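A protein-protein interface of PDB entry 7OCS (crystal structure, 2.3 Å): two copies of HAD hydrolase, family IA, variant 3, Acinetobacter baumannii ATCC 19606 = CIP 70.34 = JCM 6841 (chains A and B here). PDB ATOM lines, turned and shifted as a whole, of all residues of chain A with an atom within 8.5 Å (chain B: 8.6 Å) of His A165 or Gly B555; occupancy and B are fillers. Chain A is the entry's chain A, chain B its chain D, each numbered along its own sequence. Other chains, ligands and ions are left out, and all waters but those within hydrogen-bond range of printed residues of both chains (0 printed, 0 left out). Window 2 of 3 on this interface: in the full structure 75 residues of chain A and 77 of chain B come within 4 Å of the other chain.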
ATOM      1  N   HIS A  11     -22.321  -8.448  22.578  1.00  0.00           N
ATOM      2  CA  HIS A  11     -21.805  -8.931  21.288  1.00  0.00           C
ATOM      3  C   HIS A  11     -22.731  -8.574  20.088  1.00  0.00           C
ATOM      4  O   HIS A  11     -22.329  -8.716  18.934  1.00  0.00           O
ATOM      5  CB  HIS A  11     -21.569 -10.451  21.338  1.00  0.00           C
ATOM      6  CG  HIS A  11     -20.428 -10.838  22.222  1.00  0.00           C
ATOM      7  ND1 HIS A  11     -19.132 -10.925  21.733  1.00  0.00           N
ATOM      8  CD2 HIS A  11     -20.414 -11.104  23.548  1.00  0.00           C
ATOM      9  CE1 HIS A  11     -18.379 -11.253  22.769  1.00  0.00           C
ATOM     10  NE2 HIS A  11     -19.107 -11.383  23.882  1.00  0.00           N
ATOM     11  N   GLY A  12     -23.956  -8.153  20.379  1.00  0.00           N
ATOM     12  CA  GLY A  12     -24.920  -7.824  19.353  1.00  0.00           C
ATOM     13  C   GLY A  12     -25.884  -6.737  19.755  1.00  0.00           C
ATOM     14  O   GLY A  12     -26.000  -6.402  20.933  1.00  0.00           O
ATOM     15  N   ILE A  14     -29.907  -5.424  18.592  1.00  0.00           N
ATOM     16  CA  ILE A  14     -31.103  -5.631  17.789  1.00  0.00           C
ATOM     17  C   ILE A  14     -32.046  -4.461  17.977  1.00  0.00           C
ATOM     18  O   ILE A  14     -32.389  -4.122  19.106  1.00  0.00           O
ATOM     19  CB  ILE A  14     -31.775  -6.979  18.125  1.00  0.00           C
ATOM     20  CG1 ILE A  14     -30.765  -8.138  18.023  1.00  0.00           C
ATOM     21  CG2 ILE A  14     -32.968  -7.209  17.220  1.00  0.00           C
ATOM     22  CD1 ILE A  14     -31.279  -9.440  18.514  1.00  0.00           C
ATOM     23  N   ARG A 113     -22.587  -7.678  16.103  1.00  0.00           N
ATOM     24  CA  ARG A 113     -23.479  -8.221  15.088  1.00  0.00           C
ATOM     25  C   ARG A 113     -24.780  -7.432  15.261  1.00  0.00           C
ATOM     26  O   ARG A 113     -25.169  -7.153  16.406  1.00  0.00           O
ATOM     27  CB  ARG A 113     -23.750  -9.717  15.345  1.00  0.00           C
ATOM     28  CG  ARG A 113     -22.507 -10.547  15.659  1.00  0.00           C
ATOM     29  CD  ARG A 113     -21.506 -10.572  14.514  1.00  0.00           C
ATOM     30  NE  ARG A 113     -20.591 -11.714  14.632  1.00  0.00           N
ATOM     31  CZ  ARG A 113     -19.594 -11.965  13.783  1.00  0.00           C
ATOM     32  NH1 ARG A 113     -19.370 -11.156  12.751  1.00  0.00           N
ATOM     33  NH2 ARG A 113     -18.817 -13.028  13.958  1.00  0.00           N
ATOM     34  N   ALA A 115     -28.951  -6.431  13.986  1.00  0.00           N
ATOM     35  CA  ALA A 115     -30.156  -6.848  13.319  1.00  0.00           C
ATOM     36  C   ALA A 115     -31.306  -5.880  13.567  1.00  0.00           C
ATOM     37  O   ALA A 115     -31.273  -5.098  14.521  1.00  0.00           O
ATOM     38  CB  ALA A 115     -30.544  -8.254  13.795  1.00  0.00           C
ATOM     39  N   ASP A 139     -26.673  -7.076   9.669  1.00  0.00           N
ATOM     40  CA  ASP A 139     -26.390  -8.404   9.134  1.00  0.00           C
ATOM     41  C   ASP A 139     -27.678  -9.164   8.853  1.00  0.00           C
ATOM     42  O   ASP A 139     -27.724  -9.985   7.938  1.00  0.00           O
ATOM     43  CB  ASP A 139     -25.565  -9.209  10.152  1.00  0.00           C
ATOM     44  CG  ASP A 139     -24.275  -8.542  10.528  1.00  0.00           C
ATOM     45  OD1 ASP A 139     -24.132  -8.149  11.707  1.00  0.00           O
ATOM     46  OD2 ASP A 139     -23.412  -8.387   9.641  1.00  0.00           O
ATOM     47  N   VAL A 140     -28.705  -8.955   9.700  1.00  0.00           N
ATOM     48  CA  VAL A 140     -29.962  -9.680   9.644  1.00  0.00           C
ATOM     49  C   VAL A 140     -31.150  -8.709   9.769  1.00  0.00           C
ATOM     50  O   VAL A 140     -31.059  -7.708  10.463  1.00  0.00           O
ATOM     51  CB  VAL A 140     -29.966 -10.755  10.796  1.00  0.00           C
ATOM     52  CG1 VAL A 140     -31.378 -11.182  11.186  1.00  0.00           C
ATOM     53  CG2 VAL A 140     -29.114 -11.962  10.426  1.00  0.00           C
ATOM     54  N   LEU A 158     -36.006 -13.348  19.497  1.00  0.00           N
ATOM     55  CA  LEU A 158     -35.287 -14.619  19.639  1.00  0.00           C
ATOM     56  C   LEU A 158     -34.750 -15.093  18.280  1.00  0.00           C
ATOM     57  O   LEU A 158     -33.683 -15.694  18.223  1.00  0.00           O
ATOM     58  CB  LEU A 158     -36.221 -15.698  20.217  1.00  0.00           C
ATOM     59  CG  LEU A 158     -36.550 -15.559  21.692  1.00  0.00           C
ATOM     60  CD1 LEU A 158     -37.676 -16.508  22.091  1.00  0.00           C
ATOM     61  CD2 LEU A 158     -35.331 -15.795  22.542  1.00  0.00           C
ATOM     62  N   LYS A 159     -35.508 -14.820  17.188  1.00  0.00           N
ATOM     63  CA  LYS A 159     -35.155 -15.204  15.824  1.00  0.00           C
ATOM     64  C   LYS A 159     -34.070 -14.295  15.270  1.00  0.00           C
ATOM     65  O   LYS A 159     -33.169 -14.771  14.581  1.00  0.00           O
ATOM     66  CB  LYS A 159     -36.397 -15.177  14.922  1.00  0.00           C
ATOM     67  CG  LYS A 159     -36.168 -15.771  13.549  1.00  0.00           C
ATOM     68  CD  LYS A 159     -37.401 -15.605  12.668  1.00  0.00           C
ATOM     69  CE  LYS A 159     -37.195 -16.171  11.289  1.00  0.00           C
ATOM     70  NZ  LYS A 159     -38.407 -16.000  10.444  1.00  0.00           N
ATOM     71  N   ALA A 160     -34.128 -12.987  15.592  1.00  0.00           N
ATOM     72  CA  ALA A 160     -33.087 -12.053  15.166  1.00  0.00           C
ATOM     73  C   ALA A 160     -31.770 -12.414  15.852  1.00  0.00           C
ATOM     74  O   ALA A 160     -30.730 -12.446  15.199  1.00  0.00           O
ATOM     75  CB  ALA A 160     -33.485 -10.623  15.511  1.00  0.00           C
ATOM     76  N   ALA A 161     -31.820 -12.746  17.158  1.00  0.00           N
ATOM     77  CA  ALA A 161     -30.620 -13.127  17.912  1.00  0.00           C
ATOM     78  C   ALA A 161     -30.071 -14.453  17.397  1.00  0.00           C
ATOM     79  O   ALA A 161     -28.864 -14.583  17.206  1.00  0.00           O
ATOM     80  CB  ALA A 161     -30.936 -13.227  19.403  1.00  0.00           C
ATOM     81  N   SER A 162     -30.955 -15.410  17.114  1.00  0.00           N
ATOM     82  CA  SER A 162     -30.560 -16.701  16.582  1.00  0.00           C
ATOM     83  C   SER A 162     -29.903 -16.547  15.214  1.00  0.00           C
ATOM     84  O   SER A 162     -28.903 -17.198  14.946  1.00  0.00           O
ATOM     85  CB  SER A 162     -31.767 -17.626  16.486  1.00  0.00           C
ATOM     86  OG  SER A 162     -31.423 -18.868  15.897  1.00  0.00           O
ATOM     87  N   GLN A 163     -30.430 -15.642  14.366  1.00  0.00           N
ATOM     88  CA  GLN A 163     -29.845 -15.395  13.050  1.00  0.00           C
ATOM     89  C   GLN A 163     -28.508 -14.655  13.128  1.00  0.00           C
ATOM     90  O   GLN A 163     -27.673 -14.827  12.246  1.00  0.00           O
ATOM     91  CB  GLN A 163     -30.831 -14.698  12.123  1.00  0.00           C
ATOM     92  CG  GLN A 163     -31.891 -15.645  11.579  1.00  0.00           C
ATOM     93  CD  GLN A 163     -32.627 -15.039  10.424  1.00  0.00           C
ATOM     94  OE1 GLN A 163     -33.465 -14.140  10.587  1.00  0.00           O
ATOM     95  NE2 GLN A 163     -32.331 -15.509   9.224  1.00  0.00           N
ATOM     96  N   LEU A 164     -28.278 -13.869  14.204  1.00  0.00           N
ATOM     97  CA  LEU A 164     -26.973 -13.221  14.431  1.00  0.00           C
ATOM     98  C   LEU A 164     -25.943 -14.230  15.049  1.00  0.00           C
ATOM     99  O   LEU A 164     -24.766 -13.901  15.158  1.00  0.00           O
ATOM    100  CB  LEU A 164     -27.113 -12.019  15.379  1.00  0.00           C
ATOM    101  CG  LEU A 164     -27.868 -10.800  14.860  1.00  0.00           C
ATOM    102  CD1 LEU A 164     -27.935  -9.708  15.939  1.00  0.00           C
ATOM    103  CD2 LEU A 164     -27.223 -10.250  13.604  1.00  0.00           C
ATOM    104  N   HIS A 165     -26.423 -15.434  15.487  1.00  0.00           N
ATOM    105  CA  HIS A 165     -25.644 -16.499  16.134  1.00  0.00           C
ATOM    106  C   HIS A 165     -25.165 -16.076  17.514  1.00  0.00           C
ATOM    107  O   HIS A 165     -24.027 -16.339  17.901  1.00  0.00           O
ATOM    108  CB  HIS A 165     -24.495 -16.992  15.250  1.00  0.00           C
ATOM    109  CG  HIS A 165     -24.911 -17.300  13.848  1.00  0.00           C
ATOM    110  ND1 HIS A 165     -24.033 -17.190  12.803  1.00  0.00           N
ATOM    111  CD2 HIS A 165     -26.118 -17.678  13.363  1.00  0.00           C
ATOM    112  CE1 HIS A 165     -24.720 -17.506  11.721  1.00  0.00           C
ATOM    113  NE2 HIS A 165     -25.973 -17.823  12.014  1.00  0.00           N
ATOM    114  N   LEU A 166     -26.038 -15.407  18.247  1.00  0.00           N
ATOM    115  CA  LEU A 166     -25.769 -14.945  19.596  1.00  0.00           C
ATOM    116  C   LEU A 166     -26.954 -15.268  20.469  1.00  0.00           C
ATOM    117  O   LEU A 166     -28.092 -15.313  19.985  1.00  0.00           O
ATOM    118  CB  LEU A 166     -25.574 -13.420  19.612  1.00  0.00           C
ATOM    119  CG  LEU A 166     -24.445 -12.873  18.793  1.00  0.00           C
ATOM    120  CD1 LEU A 166     -24.559 -11.381  18.670  1.00  0.00           C
ATOM    121  CD2 LEU A 166     -23.101 -13.263  19.382  1.00  0.00           C
ATOM    122  N   ASP A 167     -26.713 -15.443  21.763  1.00  0.00           N
ATOM    123  CA  ASP A 167     -27.794 -15.619  22.714  1.00  0.00           C
ATOM    124  C   ASP A 167     -28.456 -14.254  22.896  1.00  0.00           C
ATOM    125  O   ASP A 167     -27.791 -13.223  22.766  1.00  0.00           O
ATOM    126  CB  ASP A 167     -27.251 -16.128  24.053  1.00  0.00           C
ATOM    127  CG  ASP A 167     -26.641 -17.510  23.973  1.00  0.00           C
ATOM    128  OD1 ASP A 167     -27.126 -18.327  23.163  1.00  0.00           O
ATOM    129  OD2 ASP A 167     -25.682 -17.780  24.729  1.00  0.00           O
ATOM    130  N   ALA A 168     -29.744 -14.234  23.182  1.00  0.00           N
ATOM    131  CA  ALA A 168     -30.477 -12.981  23.364  1.00  0.00           C
ATOM    132  C   ALA A 168     -29.881 -12.115  24.485  1.00  0.00           C
ATOM    133  O   ALA A 168     -29.849 -10.891  24.354  1.00  0.00           O
ATOM    134  CB  ALA A 168     -31.948 -13.267  23.634  1.00  0.00           C
ATOM    135  N   GLN A 170     -26.777 -11.691  25.161  1.00  0.00           N
ATOM    136  CA  GLN A 170     -25.571 -10.999  24.688  1.00  0.00           C
ATOM    137  C   GLN A 170     -25.946  -9.819  23.738  1.00  0.00           C
ATOM    138  O   GLN A 170     -25.056  -9.207  23.155  1.00  0.00           O
ATOM    139  CB  GLN A 170     -24.634 -11.968  23.952  1.00  0.00           C
ATOM    140  CG  GLN A 170     -24.393 -13.288  24.683  1.00  0.00           C
ATOM    141  CD  GLN A 170     -23.580 -14.214  23.826  1.00  0.00           C
ATOM    142  OE1 GLN A 170     -24.058 -14.757  22.820  1.00  0.00           O
ATOM    143  NE2 GLN A 170     -22.332 -14.396  24.188  1.00  0.00           N
ATOM    144  N   CYS A 171     -27.264  -9.522  23.577  1.00  0.00           N
ATOM    145  CA  CYS A 171     -27.737  -8.496  22.674  1.00  0.00           C
ATOM    146  C   CYS A 171     -28.396  -7.371  23.382  1.00  0.00           C
ATOM    147  O   CYS A 171     -29.301  -7.596  24.181  1.00  0.00           O
ATOM    148  CB  CYS A 171     -28.682  -9.093  21.629  1.00  0.00           C
ATOM    149  SG  CYS A 171     -27.942 -10.368  20.584  1.00  0.00           S
ATOM    150  N   TYR B 547     -29.653 -28.977   9.241  1.00  0.00           N
ATOM    151  CA  TYR B 547     -29.652 -27.675   8.579  1.00  0.00           C
ATOM    152  C   TYR B 547     -29.474 -27.812   7.069  1.00  0.00           C
ATOM    153  O   TYR B 547     -28.925 -28.808   6.594  1.00  0.00           O
ATOM    154  CB  TYR B 547     -28.559 -26.762   9.169  1.00  0.00           C
ATOM    155  CG  TYR B 547     -28.568 -26.708  10.680  1.00  0.00           C
ATOM    156  CD1 TYR B 547     -29.626 -26.134  11.369  1.00  0.00           C
ATOM    157  CD2 TYR B 547     -27.527 -27.248  11.421  1.00  0.00           C
ATOM    158  CE1 TYR B 547     -29.647 -26.093  12.758  1.00  0.00           C
ATOM    159  CE2 TYR B 547     -27.534 -27.210  12.811  1.00  0.00           C
ATOM    160  CZ  TYR B 547     -28.597 -26.630  13.475  1.00  0.00           C
ATOM    161  OH  TYR B 547     -28.612 -26.587  14.847  1.00  0.00           O
ATOM    162  N   SER B 549     -28.244 -24.943   5.209  1.00  0.00           N
ATOM    163  CA  SER B 549     -27.358 -23.859   4.815  1.00  0.00           C
ATOM    164  C   SER B 549     -26.120 -23.792   5.719  1.00  0.00           C
ATOM    165  O   SER B 549     -26.178 -24.185   6.887  1.00  0.00           O
ATOM    166  CB  SER B 549     -28.101 -22.528   4.843  1.00  0.00           C
ATOM    167  OG  SER B 549     -27.238 -21.458   4.503  1.00  0.00           O
ATOM    168  N   ILE B 550     -25.002 -23.293   5.171  1.00  0.00           N
ATOM    169  CA  ILE B 550     -23.748 -23.152   5.911  1.00  0.00           C
ATOM    170  C   ILE B 550     -23.896 -22.091   7.010  1.00  0.00           C
ATOM    171  O   ILE B 550     -23.516 -22.328   8.157  1.00  0.00           O
ATOM    172  CB  ILE B 550     -22.587 -22.817   4.924  1.00  0.00           C
ATOM    173  CG1 ILE B 550     -22.251 -24.033   4.038  1.00  0.00           C
ATOM    174  CG2 ILE B 550     -21.342 -22.308   5.662  1.00  0.00           C
ATOM    175  CD1 ILE B 550     -21.784 -25.256   4.811  1.00  0.00           C
ATOM    176  N   GLY B 551     -24.491 -20.957   6.649  1.00  0.00           N
ATOM    177  CA  GLY B 551     -24.718 -19.845   7.562  1.00  0.00           C
ATOM    178  C   GLY B 551     -25.683 -20.184   8.676  1.00  0.00           C
ATOM    179  O   GLY B 551     -25.505 -19.739   9.808  1.00  0.00           O
ATOM    180  N   VAL B 552     -26.700 -20.992   8.370  1.00  0.00           N
ATOM    181  CA  VAL B 552     -27.677 -21.428   9.372  1.00  0.00           C
ATOM    182  C   VAL B 552     -26.999 -22.370  10.398  1.00  0.00           C
ATOM    183  O   VAL B 552     -27.247 -22.260  11.608  1.00  0.00           O
ATOM    184  CB  VAL B 552     -28.906 -22.088   8.690  1.00  0.00           C
ATOM    185  CG1 VAL B 552     -29.791 -22.797   9.703  1.00  0.00           C
ATOM    186  CG2 VAL B 552     -29.705 -21.056   7.901  1.00  0.00           C
ATOM    187  N   ALA B 553     -26.082 -23.239   9.912  1.00  0.00           N
ATOM    188  CA  ALA B 553     -25.338 -24.178  10.758  1.00  0.00           C
ATOM    189  C   ALA B 553     -24.402 -23.474  11.726  1.00  0.00           C
ATOM    190  O   ALA B 553     -24.126 -24.011  12.795  1.00  0.00           O
ATOM    191  CB  ALA B 553     -24.554 -25.141   9.901  1.00  0.00           C
ATOM    192  N   MET B 554     -23.907 -22.269  11.360  1.00  0.00           N
ATOM    193  CA  MET B 554     -23.028 -21.484  12.237  1.00  0.00           C
ATOM    194  C   MET B 554     -23.728 -21.060  13.557  1.00  0.00           C
ATOM    195  O   MET B 554     -23.052 -20.803  14.555  1.00  0.00           O
ATOM    196  CB  MET B 554     -22.460 -20.266  11.495  1.00  0.00           C
ATOM    197  CG  MET B 554     -21.544 -20.636  10.345  1.00  0.00           C
ATOM    198  SD  MET B 554     -20.028 -21.488  10.865  1.00  0.00           S
ATOM    199  CE  MET B 554     -20.248 -23.037  10.049  1.00  0.00           C
ATOM    200  N   GLY B 555     -25.070 -21.031  13.548  1.00  0.00           N
ATOM    201  CA  GLY B 555     -25.873 -20.749  14.730  1.00  0.00           C
ATOM    202  C   GLY B 555     -25.719 -21.821  15.794  1.00  0.00           C
ATOM    203  O   GLY B 555     -25.768 -21.524  16.990  1.00  0.00           O
ATOM    204  N   ASP B 556     -25.501 -23.077  15.364  1.00  0.00           N
ATOM    205  CA  ASP B 556     -25.260 -24.186  16.276  1.00  0.00           C
ATOM    206  C   ASP B 556     -23.848 -24.028  16.834  1.00  0.00           C
ATOM    207  O   ASP B 556     -22.887 -23.963  16.067  1.00  0.00           O
ATOM    208  CB  ASP B 556     -25.400 -25.528  15.531  1.00  0.00           C
ATOM    209  CG  ASP B 556     -25.542 -26.748  16.429  1.00  0.00           C
ATOM    210  OD1 ASP B 556     -25.102 -26.682  17.601  1.00  0.00           O
ATOM    211  OD2 ASP B 556     -26.083 -27.769  15.957  1.00  0.00           O
ATOM    212  N   HIS B 557     -23.726 -23.932  18.163  1.00  0.00           N
ATOM    213  CA  HIS B 557     -22.437 -23.729  18.820  1.00  0.00           C
ATOM    214  C   HIS B 557     -21.454 -24.885  18.585  1.00  0.00           C
ATOM    215  O   HIS B 557     -20.244 -24.660  18.561  1.00  0.00           O
ATOM    216  CB  HIS B 557     -22.630 -23.463  20.329  1.00  0.00           C
ATOM    217  CG  HIS B 557     -22.989 -24.683  21.119  1.00  0.00           C
ATOM    218  ND1 HIS B 557     -24.126 -25.421  20.832  1.00  0.00           N
ATOM    219  CD2 HIS B 557     -22.339 -25.265  22.156  1.00  0.00           C
ATOM    220  CE1 HIS B 557     -24.133 -26.421  21.701  1.00  0.00           C
ATOM    221  NE2 HIS B 557     -23.080 -26.367  22.521  1.00  0.00           N
ATOM    222  N   LEU B 558     -21.965 -26.113  18.416  1.00  0.00           N
ATOM    223  CA  LEU B 558     -21.099 -27.268  18.180  1.00  0.00           C
ATOM    224  C   LEU B 558     -20.565 -27.304  16.735  1.00  0.00           C
ATOM    225  O   LEU B 558     -19.485 -27.841  16.495  1.00  0.00           O
ATOM    226  CB  LEU B 558     -21.818 -28.575  18.538  1.00  0.00           C
ATOM    227  CG  LEU B 558     -22.314 -28.662  19.986  1.00  0.00           C
ATOM    228  CD1 LEU B 558     -23.115 -29.920  20.210  1.00  0.00           C
ATOM    229  CD2 LEU B 558     -21.155 -28.586  20.973  1.00  0.00           C
ATOM    230  N   VAL B 559     -21.301 -26.708  15.782  1.00  0.00           N
ATOM    231  CA  VAL B 559     -20.854 -26.643  14.402  1.00  0.00           C
ATOM    232  C   VAL B 559     -19.802 -25.526  14.241  1.00  0.00           C
ATOM    233  O   VAL B 559     -18.813 -25.714  13.534  1.00  0.00           O
ATOM    234  CB  VAL B 559     -22.043 -26.475  13.427  1.00  0.00           C
ATOM    235  CG1 VAL B 559     -21.562 -26.394  11.981  1.00  0.00           C
ATOM    236  CG2 VAL B 559     -23.050 -27.607  13.599  1.00  0.00           C
ATOM    237  N   LYS B 560     -19.984 -24.394  14.946  1.00  0.00           N
ATOM    238  CA  LYS B 560     -19.028 -23.286  14.899  1.00  0.00           C
ATOM    239  C   LYS B 560     -17.670 -23.694  15.521  1.00  0.00           C
ATOM    240  O   LYS B 560     -16.617 -23.425  14.934  1.00  0.00           O
ATOM    241  CB  LYS B 560     -19.601 -22.044  15.602  1.00  0.00           C
ATOM    242  CG  LYS B 560     -18.665 -20.843  15.575  1.00  0.00           C
ATOM    243  CD  LYS B 560     -19.417 -19.531  15.729  1.00  0.00           C
ATOM    244  CE  LYS B 560     -18.473 -18.351  15.740  1.00  0.00           C
ATOM    245  NZ  LYS B 560     -19.198 -17.058  15.593  1.00  0.00           N
ATOM    246  N   ALA B 561     -17.700 -24.382  16.682  1.00  0.00           N
ATOM    247  CA  ALA B 561     -16.478 -24.852  17.343  1.00  0.00           C
ATOM    248  C   ALA B 561     -15.756 -25.888  16.479  1.00  0.00           C
ATOM    249  O   ALA B 561     -14.532 -25.887  16.420  1.00  0.00           O
ATOM    250  CB  ALA B 561     -16.813 -25.451  18.696  1.00  0.00           C
ATOM    251  N   LEU B 593     -13.306 -18.412   8.423  1.00  0.00           N
ATOM    252  CA  LEU B 593     -14.294 -18.437   9.497  1.00  0.00           C
ATOM    253  C   LEU B 593     -15.214 -17.223   9.439  1.00  0.00           C
ATOM    254  O   LEU B 593     -16.411 -17.351   9.699  1.00  0.00           O
ATOM    255  CB  LEU B 593     -13.603 -18.516  10.866  1.00  0.00           C
ATOM    256  CG  LEU B 593     -12.861 -19.821  11.158  1.00  0.00           C
ATOM    257  CD1 LEU B 593     -11.987 -19.685  12.376  1.00  0.00           C
ATOM    258  CD2 LEU B 593     -13.830 -20.973  11.330  1.00  0.00           C
ATOM    259  N   CYS B 596     -17.708 -17.787   6.485  1.00  0.00           N
ATOM    260  CA  CYS B 596     -18.679 -18.865   6.718  1.00  0.00           C
ATOM    261  C   CYS B 596     -19.808 -18.437   7.667  1.00  0.00           C
ATOM    262  O   CYS B 596     -20.912 -18.972   7.585  1.00  0.00           O
ATOM    263  CB  CYS B 596     -17.981 -20.127   7.218  1.00  0.00           C
ATOM    264  SG  CYS B 596     -17.372 -21.207   5.899  1.00  0.00           S
ATOM    265  N   GLU B 597     -19.520 -17.472   8.569  1.00  0.00           N
ATOM    266  CA  GLU B 597     -20.455 -16.956   9.567  1.00  0.00           C
ATOM    267  C   GLU B 597     -21.863 -16.672   9.015  1.00  0.00           C
ATOM    268  O   GLU B 597     -22.821 -17.269   9.483  1.00  0.00           O
ATOM    269  CB  GLU B 597     -19.867 -15.711  10.269  1.00  0.00           C
ATOM    270  CG  GLU B 597     -20.716 -15.201  11.419  1.00  0.00           C
ATOM    271  CD  GLU B 597     -20.740 -16.110  12.631  1.00  0.00           C
ATOM    272  OE1 GLU B 597     -21.790 -16.169  13.308  1.00  0.00           O
ATOM    273  OE2 GLU B 597     -19.710 -16.764  12.906  1.00  0.00           O
ATOM    274  N   TYR B 598     -21.982 -15.801   7.997  1.00  0.00           N
ATOM    275  CA  TYR B 598     -23.286 -15.472   7.430  1.00  0.00           C
ATOM    276  C   TYR B 598     -23.420 -15.923   5.971  1.00  0.00           C
ATOM    277  O   TYR B 598     -23.940 -15.178   5.138  1.00  0.00           O
ATOM    278  CB  TYR B 598     -23.584 -13.968   7.575  1.00  0.00           C
ATOM    279  CG  TYR B 598     -23.666 -13.514   9.013  1.00  0.00           C
ATOM    280  CD1 TYR B 598     -24.591 -14.067   9.885  1.00  0.00           C
ATOM    281  CD2 TYR B 598     -22.827 -12.523   9.499  1.00  0.00           C
ATOM    282  CE1 TYR B 598     -24.668 -13.658  11.208  1.00  0.00           C
ATOM    283  CE2 TYR B 598     -22.902 -12.099  10.818  1.00  0.00           C
ATOM    284  CZ  TYR B 598     -23.825 -12.670  11.671  1.00  0.00           C
ATOM    285  OH  TYR B 598     -23.904 -12.263  12.976  1.00  0.00           O
ATOM    286  N   ALA B 599     -22.989 -17.156   5.665  1.00  0.00           N
ATOM    287  CA  ALA B 599     -23.089 -17.686   4.302  1.00  0.00           C
ATOM    288  C   ALA B 599     -24.455 -18.366   4.071  1.00  0.00           C
ATOM    289  O   ALA B 599     -24.515 -19.554   3.736  1.00  0.00           O
ATOM    290  CB  ALA B 599     -21.944 -18.662   4.028  1.00  0.00           C
ATOM    291  N   PHE B 600     -25.552 -17.615   4.277  1.00  0.00           N
ATOM    292  CA  PHE B 600     -26.909 -18.139   4.097  1.00  0.00           C
ATOM    293  C   PHE B 600     -27.215 -18.464   2.621  1.00  0.00           C
ATOM    294  O   PHE B 600     -28.013 -19.357   2.341  1.00  0.00           O
ATOM    295  CB  PHE B 600     -27.952 -17.151   4.649  1.00  0.00           C
ATOM    296  CG  PHE B 600     -27.756 -16.767   6.098  1.00  0.00           C
ATOM    297  CD1 PHE B 600     -27.897 -17.705   7.106  1.00  0.00           C
ATOM    298  CD2 PHE B 600     -27.480 -15.460   6.453  1.00  0.00           C
ATOM    299  CE1 PHE B 600     -27.742 -17.346   8.439  1.00  0.00           C
ATOM    300  CE2 PHE B 600     -27.329 -15.104   7.787  1.00  0.00           C
ATOM    301  CZ  PHE B 600     -27.457 -16.049   8.771  1.00  0.00           C
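The guanidinium group (NH2) of Arg A113 lies within salt-bridge range of the side-chain carboxylate (OE2) of Glu B597, at 3.98 Å. The side-chain hydroxyl of Tyr B598 is in hydrogen-bond range of the backbone carbonyl oxygen of Leu A164 (2.9 Å). NE2 of His A165 lies within hydrogen-bond range of O of Gly B551. A ring nitrogen (ND1) of His A165 lies within hydrogen-bond range of the side-chain carboxylate of Glu B597.
The side-chain amino group (NZ) of Lys B560 lies within salt-bridge range of the side-chain carboxylate (OE2) of Glu B597, 2.8 Å away. The backbone carbonyl oxygen (O) of Ala B599 lies within hydrogen-bond range of the backbone NH (N) of Gly B551 (3.2 Å). The backbone carbonyl oxygen of His A11 is in hydrogen-bond range of the backbone NH of Arg A113 (3.0 Å). The backbone carbonyl oxygen (O) of Gln A163 sits close to a ring nitrogen (NE2) of His A165. OG of Ser B549 sits at hydrogen-bond distance from O of Phe B600 (3.1 Å).
CD of Arg A113 touches OH of Tyr B598, 3.3 Å away. CG of Asp A139 touches CE2 of Tyr B598 (3.8 Å). Gln A163 touches Tyr B598 (O to CE1, 3.4 Å). Phe B600 touches Gln A163 (CZ to O, 3.7 Å). His A165 touches Met B554 (CE1 to CB, 3.6 Å). Gly B555 touches His A165. His A165 touches Tyr B598. Phe B600 touches His A165 (CZ to NE2, 3.98 Å).
His A11 touches none of the printed residues of chain B. Of the printed residues of chain B, Gln A163 touches Tyr B598 (3.4 Å) and Phe B600 (3.7 Å). Printed residues of chain B within 4 Å of Leu A164: Tyr B598. Of the printed residues of chain B, His A165 touches Gly B551 (3.0 Å), Met B554 (3.6 Å), Gly B555 (3.4 Å), Glu B597 (2.5 Å), Tyr B598 (3.9 Å) and Phe B600 (3.98 Å). Printed residues of chain A within 4 Å of Met B554: His A165 (3.6 Å). Of chain A, only His A165 (3.4 Å) comes within 4 Å of Gly B555. Val B559 touches none of the printed residues of chain A. Of the printed residues of chain A, Tyr B598 touches Arg A113 (3.3 Å), Asp A139 (3.8 Å), Gln A163 (3.4 Å), Leu A164 (2.9 Å) and His A165 (3.9 Å). Printed residues of chain A within 4 Å of Phe B600: Gln A163 (3.7 Å) and His A165 (3.98 Å). The nearest printed residue of chain B that does not touch His A165 is Val B552 (4.6 Å). The nearest printed residue of chain A that does not touch Met B554 is Ser A162 (6.6 Å).
Hydrophobic or aromatic side chains of chain A within 4 Å of the printed part of chain B: Leu A164 and His A165. Hydrophobic or aromatic side chains of chain B that line the printed part of chain A: Met B554, Tyr B598 and Phe B600. Among the printed residues, 12 pairs touch across the chains. Among the printed residues, Asp or Glu carboxylates within 4 Å of a Lys or Arg side-chain nitrogen of the other chain: Arg A113 with Glu B597.
No position is printed for both chains.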
